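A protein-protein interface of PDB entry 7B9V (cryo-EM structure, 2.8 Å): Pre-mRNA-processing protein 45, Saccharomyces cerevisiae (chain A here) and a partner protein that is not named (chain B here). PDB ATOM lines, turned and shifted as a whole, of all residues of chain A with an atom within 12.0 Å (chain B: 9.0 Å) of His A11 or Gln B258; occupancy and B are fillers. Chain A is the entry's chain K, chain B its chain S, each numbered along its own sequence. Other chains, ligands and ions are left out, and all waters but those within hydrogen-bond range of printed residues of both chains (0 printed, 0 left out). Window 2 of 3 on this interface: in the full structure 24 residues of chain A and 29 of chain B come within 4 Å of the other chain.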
ATOM      1  N   PRO A   7      21.754  27.307  -4.047  1.00  0.00           N
ATOM      2  CA  PRO A   7      20.995  28.473  -4.521  1.00  0.00           C
ATOM      3  C   PRO A   7      19.963  28.899  -3.489  1.00  0.00           C
ATOM      4  O   PRO A   7      19.615  28.097  -2.612  1.00  0.00           O
ATOM      5  CB  PRO A   7      20.332  27.955  -5.811  1.00  0.00           C
ATOM      6  CG  PRO A   7      20.184  26.514  -5.597  1.00  0.00           C
ATOM      7  CD  PRO A   7      21.388  26.093  -4.806  1.00  0.00           C
ATOM      8  N   PRO A   8      19.503  30.158  -3.502  1.00  0.00           N
ATOM      9  CA  PRO A   8      18.526  30.588  -2.498  1.00  0.00           C
ATOM     10  C   PRO A   8      17.167  29.957  -2.751  1.00  0.00           C
ATOM     11  O   PRO A   8      16.856  29.574  -3.892  1.00  0.00           O
ATOM     12  CB  PRO A   8      18.486  32.116  -2.677  1.00  0.00           C
ATOM     13  CG  PRO A   8      18.862  32.337  -4.071  1.00  0.00           C
ATOM     14  CD  PRO A   8      19.856  31.264  -4.418  1.00  0.00           C
ATOM     15  N   PRO A   9      16.344  29.780  -1.713  1.00  0.00           N
ATOM     16  CA  PRO A   9      14.990  29.259  -1.941  1.00  0.00           C
ATOM     17  C   PRO A   9      14.113  30.267  -2.672  1.00  0.00           C
ATOM     18  O   PRO A   9      14.240  31.482  -2.503  1.00  0.00           O
ATOM     19  CB  PRO A   9      14.472  28.984  -0.525  1.00  0.00           C
ATOM     20  CG  PRO A   9      15.222  29.937   0.334  1.00  0.00           C
ATOM     21  CD  PRO A   9      16.591  30.043  -0.282  1.00  0.00           C
ATOM     22  N   LYS A  10      13.209  29.737  -3.494  1.00  0.00           N
ATOM     23  CA  LYS A  10      12.257  30.549  -4.240  1.00  0.00           C
ATOM     24  C   LYS A  10      10.911  30.691  -3.549  1.00  0.00           C
ATOM     25  O   LYS A  10      10.231  31.703  -3.747  1.00  0.00           O
ATOM     26  CB  LYS A  10      12.047  29.956  -5.638  1.00  0.00           C
ATOM     27  CG  LYS A  10      13.172  30.270  -6.618  1.00  0.00           C
ATOM     28  CD  LYS A  10      12.951  29.610  -7.976  1.00  0.00           C
ATOM     29  CE  LYS A  10      11.781  30.227  -8.727  1.00  0.00           C
ATOM     30  NZ  LYS A  10      11.710  29.735 -10.133  1.00  0.00           N
ATOM     31  N   HIS A  11      10.509  29.707  -2.751  1.00  0.00           N
ATOM     32  CA  HIS A  11       9.197  29.723  -2.115  1.00  0.00           C
ATOM     33  C   HIS A  11       9.256  30.382  -0.741  1.00  0.00           C
ATOM     34  O   HIS A  11      10.335  30.681  -0.229  1.00  0.00           O
ATOM     35  CB  HIS A  11       8.652  28.300  -1.988  1.00  0.00           C
ATOM     36  CG  HIS A  11       8.604  27.554  -3.284  1.00  0.00           C
ATOM     37  ND1 HIS A  11       7.770  27.914  -4.322  1.00  0.00           N
ATOM     38  CD2 HIS A  11       9.285  26.465  -3.711  1.00  0.00           C
ATOM     39  CE1 HIS A  11       7.942  27.080  -5.332  1.00  0.00           C
ATOM     40  NE2 HIS A  11       8.855  26.191  -4.986  1.00  0.00           N
ATOM     41  N   THR B 215       9.662  26.265   9.333  1.00  0.00           N
ATOM     42  CA  THR B 215      10.414  25.917   8.121  1.00  0.00           C
ATOM     43  C   THR B 215      11.777  26.613   8.048  1.00  0.00           C
ATOM     44  O   THR B 215      12.755  26.001   7.596  1.00  0.00           O
ATOM     45  CB  THR B 215       9.570  26.181   6.856  1.00  0.00           C
ATOM     46  OG1 THR B 215      10.317  25.812   5.687  1.00  0.00           O
ATOM     47  CG2 THR B 215       9.010  27.626   6.734  1.00  0.00           C
ATOM     48  N   ARG B 219      15.359  24.684   7.930  1.00  0.00           N
ATOM     49  CA  ARG B 219      16.381  24.836   6.898  1.00  0.00           C
ATOM     50  C   ARG B 219      17.729  25.180   7.515  1.00  0.00           C
ATOM     51  O   ARG B 219      18.764  24.639   7.093  1.00  0.00           O
ATOM     52  CB  ARG B 219      15.950  25.894   5.877  1.00  0.00           C
ATOM     53  CG  ARG B 219      16.991  26.154   4.782  1.00  0.00           C
ATOM     54  CD  ARG B 219      16.510  26.985   3.613  1.00  0.00           C
ATOM     55  NE  ARG B 219      15.547  26.254   2.801  1.00  0.00           N
ATOM     56  CZ  ARG B 219      14.288  26.616   2.612  1.00  0.00           C
ATOM     57  NH1 ARG B 219      13.795  27.713   3.161  1.00  0.00           N
ATOM     58  NH2 ARG B 219      13.516  25.876   1.823  1.00  0.00           N
ATOM     59  N   ALA B 251      17.887  16.702   1.266  1.00  0.00           N
ATOM     60  CA  ALA B 251      17.392  16.797  -0.100  1.00  0.00           C
ATOM     61  C   ALA B 251      15.915  16.474  -0.187  1.00  0.00           C
ATOM     62  O   ALA B 251      15.171  17.157  -0.902  1.00  0.00           O
ATOM     63  CB  ALA B 251      18.196  15.879  -0.987  1.00  0.00           C
ATOM     64  N   HIS B 252      15.489  15.404   0.505  1.00  0.00           N
ATOM     65  CA  HIS B 252      14.080  15.029   0.480  1.00  0.00           C
ATOM     66  C   HIS B 252      13.207  16.098   1.119  1.00  0.00           C
ATOM     67  O   HIS B 252      12.080  16.335   0.661  1.00  0.00           O
ATOM     68  CB  HIS B 252      13.850  13.687   1.164  1.00  0.00           C
ATOM     69  CG  HIS B 252      14.244  12.520   0.324  1.00  0.00           C
ATOM     70  ND1 HIS B 252      13.908  12.417  -1.009  1.00  0.00           N
ATOM     71  CD2 HIS B 252      14.898  11.381   0.637  1.00  0.00           C
ATOM     72  CE1 HIS B 252      14.380  11.281  -1.491  1.00  0.00           C
ATOM     73  NE2 HIS B 252      14.981  10.632  -0.511  1.00  0.00           N
ATOM     74  N   TRP B 253      13.684  16.706   2.223  1.00  0.00           N
ATOM     75  CA  TRP B 253      12.908  17.768   2.853  1.00  0.00           C
ATOM     76  C   TRP B 253      12.783  18.973   1.938  1.00  0.00           C
ATOM     77  O   TRP B 253      11.724  19.613   1.898  1.00  0.00           O
ATOM     78  CB  TRP B 253      13.531  18.182   4.188  1.00  0.00           C
ATOM     79  CG  TRP B 253      12.739  19.276   4.841  1.00  0.00           C
ATOM     80  CD1 TRP B 253      11.573  19.143   5.529  1.00  0.00           C
ATOM     81  CD2 TRP B 253      13.046  20.678   4.844  1.00  0.00           C
ATOM     82  NE1 TRP B 253      11.131  20.369   5.960  1.00  0.00           N
ATOM     83  CE2 TRP B 253      12.020  21.329   5.555  1.00  0.00           C
ATOM     84  CE3 TRP B 253      14.090  21.444   4.317  1.00  0.00           C
ATOM     85  CZ2 TRP B 253      12.007  22.707   5.754  1.00  0.00           C
ATOM     86  CZ3 TRP B 253      14.076  22.813   4.517  1.00  0.00           C
ATOM     87  CH2 TRP B 253      13.042  23.429   5.228  1.00  0.00           C
ATOM     88  N   GLU B 254      13.885  19.348   1.267  1.00  0.00           N
ATOM     89  CA  GLU B 254      13.829  20.475   0.339  1.00  0.00           C
ATOM     90  C   GLU B 254      12.923  20.188  -0.845  1.00  0.00           C
ATOM     91  O   GLU B 254      12.299  21.108  -1.385  1.00  0.00           O
ATOM     92  CB  GLU B 254      15.220  20.880  -0.146  1.00  0.00           C
ATOM     93  CG  GLU B 254      16.050  21.648   0.868  1.00  0.00           C
ATOM     94  CD  GLU B 254      15.712  23.151   1.013  1.00  0.00           C
ATOM     95  OE1 GLU B 254      14.587  23.617   0.705  1.00  0.00           O
ATOM     96  OE2 GLU B 254      16.613  23.889   1.465  1.00  0.00           O
ATOM     97  N   ALA B 255      12.844  18.914  -1.259  1.00  0.00           N
ATOM     98  CA  ALA B 255      11.912  18.544  -2.316  1.00  0.00           C
ATOM     99  C   ALA B 255      10.473  18.649  -1.838  1.00  0.00           C
ATOM    100  O   ALA B 255       9.593  19.068  -2.597  1.00  0.00           O
ATOM    101  CB  ALA B 255      12.221  17.134  -2.811  1.00  0.00           C
ATOM    102  N   ALA B 256      10.204  18.209  -0.601  1.00  0.00           N
ATOM    103  CA  ALA B 256       8.860  18.342  -0.045  1.00  0.00           C
ATOM    104  C   ALA B 256       8.476  19.800   0.187  1.00  0.00           C
ATOM    105  O   ALA B 256       7.289  20.138   0.176  1.00  0.00           O
ATOM    106  CB  ALA B 256       8.749  17.550   1.258  1.00  0.00           C
ATOM    107  N   GLN B 257       9.465  20.677   0.402  1.00  0.00           N
ATOM    108  CA  GLN B 257       9.297  22.129   0.411  1.00  0.00           C
ATOM    109  C   GLN B 257       9.153  22.737  -0.998  1.00  0.00           C
ATOM    110  O   GLN B 257       8.950  23.959  -1.105  1.00  0.00           O
ATOM    111  CB  GLN B 257      10.458  22.717   1.265  1.00  0.00           C
ATOM    112  CG  GLN B 257      10.538  24.231   1.561  1.00  0.00           C
ATOM    113  CD  GLN B 257       9.239  24.750   2.161  1.00  0.00           C
ATOM    114  OE1 GLN B 257       8.974  24.609   3.352  1.00  0.00           O
ATOM    115  NE2 GLN B 257       8.381  25.288   1.298  1.00  0.00           N
ATOM    116  N   GLN B 258       9.204  21.902  -2.063  1.00  0.00           N
ATOM    117  CA  GLN B 258       9.026  22.245  -3.488  1.00  0.00           C
ATOM    118  C   GLN B 258      10.245  22.995  -4.027  1.00  0.00           C
ATOM    119  O   GLN B 258      10.151  23.754  -5.002  1.00  0.00           O
ATOM    120  CB  GLN B 258       7.709  22.990  -3.791  1.00  0.00           C
ATOM    121  CG  GLN B 258       7.049  22.776  -5.113  1.00  0.00           C
ATOM    122  CD  GLN B 258       5.852  23.676  -5.245  1.00  0.00           C
ATOM    123  OE1 GLN B 258       5.365  24.208  -4.251  1.00  0.00           O
ATOM    124  NE2 GLN B 258       5.396  23.896  -6.471  1.00  0.00           N
ATOM    125  N   GLU B 259      11.403  22.794  -3.398  1.00  0.00           N
ATOM    126  CA  GLU B 259      12.650  23.378  -3.889  1.00  0.00           C
ATOM    127  C   GLU B 259      13.499  22.317  -4.579  1.00  0.00           C
ATOM    128  O   GLU B 259      14.494  21.819  -4.049  1.00  0.00           O
ATOM    129  CB  GLU B 259      13.423  24.033  -2.746  1.00  0.00           C
ATOM    130  CG  GLU B 259      12.727  25.188  -2.035  1.00  0.00           C
ATOM    131  CD  GLU B 259      12.590  26.478  -2.857  1.00  0.00           C
ATOM    132  OE1 GLU B 259      13.095  26.586  -3.999  1.00  0.00           O
ATOM    133  OE2 GLU B 259      11.952  27.418  -2.337  1.00  0.00           O
ATOM    134  N   TYR B 260      13.036  21.962  -5.782  1.00  0.00           N
ATOM    135  CA  TYR B 260      13.691  20.913  -6.550  1.00  0.00           C
ATOM    136  C   TYR B 260      15.075  21.349  -7.018  1.00  0.00           C
ATOM    137  O   TYR B 260      15.991  20.515  -7.094  1.00  0.00           O
ATOM    138  CB  TYR B 260      12.819  20.523  -7.739  1.00  0.00           C
ATOM    139  CG  TYR B 260      11.435  20.106  -7.316  1.00  0.00           C
ATOM    140  CD1 TYR B 260      11.245  18.963  -6.552  1.00  0.00           C
ATOM    141  CD2 TYR B 260      10.317  20.853  -7.676  1.00  0.00           C
ATOM    142  CE1 TYR B 260       9.981  18.575  -6.150  1.00  0.00           C
ATOM    143  CE2 TYR B 260       9.043  20.468  -7.280  1.00  0.00           C
ATOM    144  CZ  TYR B 260       8.885  19.327  -6.518  1.00  0.00           C
ATOM    145  OH  TYR B 260       7.625  18.942  -6.116  1.00  0.00           O
ATOM    146  N   GLU B 261      15.236  22.644  -7.335  1.00  0.00           N
ATOM    147  CA  GLU B 261      16.536  23.160  -7.755  1.00  0.00           C
ATOM    148  C   GLU B 261      17.562  23.073  -6.628  1.00  0.00           C
ATOM    149  O   GLU B 261      18.691  22.615  -6.845  1.00  0.00           O
ATOM    150  CB  GLU B 261      16.399  24.611  -8.229  1.00  0.00           C
ATOM    151  CG  GLU B 261      17.694  25.251  -8.763  1.00  0.00           C
ATOM    152  CD  GLU B 261      18.310  24.554  -9.990  1.00  0.00           C
ATOM    153  OE1 GLU B 261      17.598  23.864 -10.759  1.00  0.00           O
ATOM    154  OE2 GLU B 261      19.536  24.687 -10.180  1.00  0.00           O
ATOM    155  N   ARG B 262      17.194  23.569  -5.430  1.00  0.00           N
ATOM    156  CA  ARG B 262      18.109  23.565  -4.285  1.00  0.00           C
ATOM    157  C   ARG B 262      18.485  22.147  -3.876  1.00  0.00           C
ATOM    158  O   ARG B 262      19.654  21.864  -3.574  1.00  0.00           O
ATOM    159  CB  ARG B 262      17.464  24.294  -3.102  1.00  0.00           C
ATOM    160  CG  ARG B 262      18.437  24.823  -2.049  1.00  0.00           C
ATOM    161  CD  ARG B 262      17.766  25.851  -1.143  1.00  0.00           C
ATOM    162  NE  ARG B 262      18.746  26.663  -0.425  1.00  0.00           N
ATOM    163  CZ  ARG B 262      19.271  26.375   0.759  1.00  0.00           C
ATOM    164  NH1 ARG B 262      18.939  25.278   1.417  1.00  0.00           N
ATOM    165  NH2 ARG B 262      20.163  27.206   1.291  1.00  0.00           N
ATOM    166  N   SER B 263      17.487  21.254  -3.834  1.00  0.00           N
ATOM    167  CA  SER B 263      17.722  19.870  -3.447  1.00  0.00           C
ATOM    168  C   SER B 263      18.614  19.149  -4.444  1.00  0.00           C
ATOM    169  O   SER B 263      19.482  18.359  -4.050  1.00  0.00           O
ATOM    170  CB  SER B 263      16.387  19.156  -3.291  1.00  0.00           C
ATOM    171  OG  SER B 263      15.639  19.277  -4.477  1.00  0.00           O
ATOM    172  N   PHE B 287      16.742   9.916  -5.250  1.00  0.00           N
ATOM    173  CA  PHE B 287      16.106  11.224  -5.401  1.00  0.00           C
ATOM    174  C   PHE B 287      15.644  11.435  -6.828  1.00  0.00           C
ATOM    175  O   PHE B 287      14.525  11.916  -7.058  1.00  0.00           O
ATOM    176  CB  PHE B 287      17.069  12.343  -4.992  1.00  0.00           C
ATOM    177  CG  PHE B 287      16.494  13.730  -5.154  1.00  0.00           C
ATOM    178  CD1 PHE B 287      15.748  14.288  -4.136  1.00  0.00           C
ATOM    179  CD2 PHE B 287      16.767  14.504  -6.288  1.00  0.00           C
ATOM    180  CE1 PHE B 287      15.216  15.550  -4.269  1.00  0.00           C
ATOM    181  CE2 PHE B 287      16.237  15.766  -6.426  1.00  0.00           C
ATOM    182  CZ  PHE B 287      15.465  16.284  -5.411  1.00  0.00           C
ATOM    183  N   PHE B 291      11.962  12.257  -8.257  1.00  0.00           N
ATOM    184  CA  PHE B 291      11.695  13.614  -8.744  1.00  0.00           C
ATOM    185  C   PHE B 291      12.515  13.899  -9.997  1.00  0.00           C
ATOM    186  O   PHE B 291      13.690  13.547 -10.072  1.00  0.00           O
ATOM    187  CB  PHE B 291      12.027  14.715  -7.709  1.00  0.00           C
ATOM    188  CG  PHE B 291      11.369  14.530  -6.362  1.00  0.00           C
ATOM    189  CD1 PHE B 291      11.963  13.759  -5.372  1.00  0.00           C
ATOM    190  CD2 PHE B 291      10.125  15.083  -6.114  1.00  0.00           C
ATOM    191  CE1 PHE B 291      11.346  13.576  -4.141  1.00  0.00           C
ATOM    192  CE2 PHE B 291       9.498  14.905  -4.892  1.00  0.00           C
ATOM    193  CZ  PHE B 291      10.108  14.152  -3.904  1.00  0.00           C
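NE of Arg B262 sits at hydrogen-bond distance from O of Pro A7, 2.8 Å away.
OE2 of Glu B259 is in hydrogen-bond range of N of Lys A10 (2.9 Å).
The backbone carbonyl oxygen of Gln B258 sits at hydrogen-bond distance from a ring nitrogen (NE2) of His A11 (2.8 Å).
OE2 of Glu B259 sits at hydrogen-bond distance from N of His A11.
The side-chain hydroxyl (OG1) of Thr B215 is in hydrogen-bond range of the side-chain amide oxygen (OE1) of Gln B257, 3.0 Å away.
The guanidinium group of Arg B219 is in salt-bridge range of the side-chain carboxylate of Glu B254.
O of Glu B254 is in hydrogen-bond range of N of Glu B259 (2.8 Å).
OE2 of Glu B254 is in salt-bridge range of NH1 of Arg B262 (2.7 Å).
O of Glu B259 lies within hydrogen-bond range of OG of Ser B263 (2.8 Å).
Arg B219 touches Pro A9.
CB of Pro A9 touches OE2 of Glu B259, at 3.5 Å.
Gln B257 touches His A11 (O to CD2, 3.6 Å).
Printed residues of chain B within 4 Å of Lys A10: Glu B259 (2.9 Å).
Of the printed residues of chain B, His A11 touches Gln B257, Gln B258 and Glu B259.
No residue of chain A comes within 4 Å of Ala B255.
Of the printed residues of chain A, Gln B258 touches His A11.
No residue of chain A comes within 4 Å of Tyr B260.
Of the printed residues of chain A, Arg B262 touches Pro A7 (2.8 Å).
The nearest printed residue of chain A that does not touch Arg B219 is His A11 (5.7 Å).
Of the 5 printed residues of chain A, 4 touch a printed residue of chain B.
Hydrophobic or aromatic side chains of chain A within 4 Å of the printed part of chain B: Pro A7, Pro A9 and His A11.
Among the printed residues, 7 pairs touch across the chains.
Among the printed residues, no Asp or Glu carboxylate lies within 4 Å of a Lys or Arg side-chain nitrogen of the other chain.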
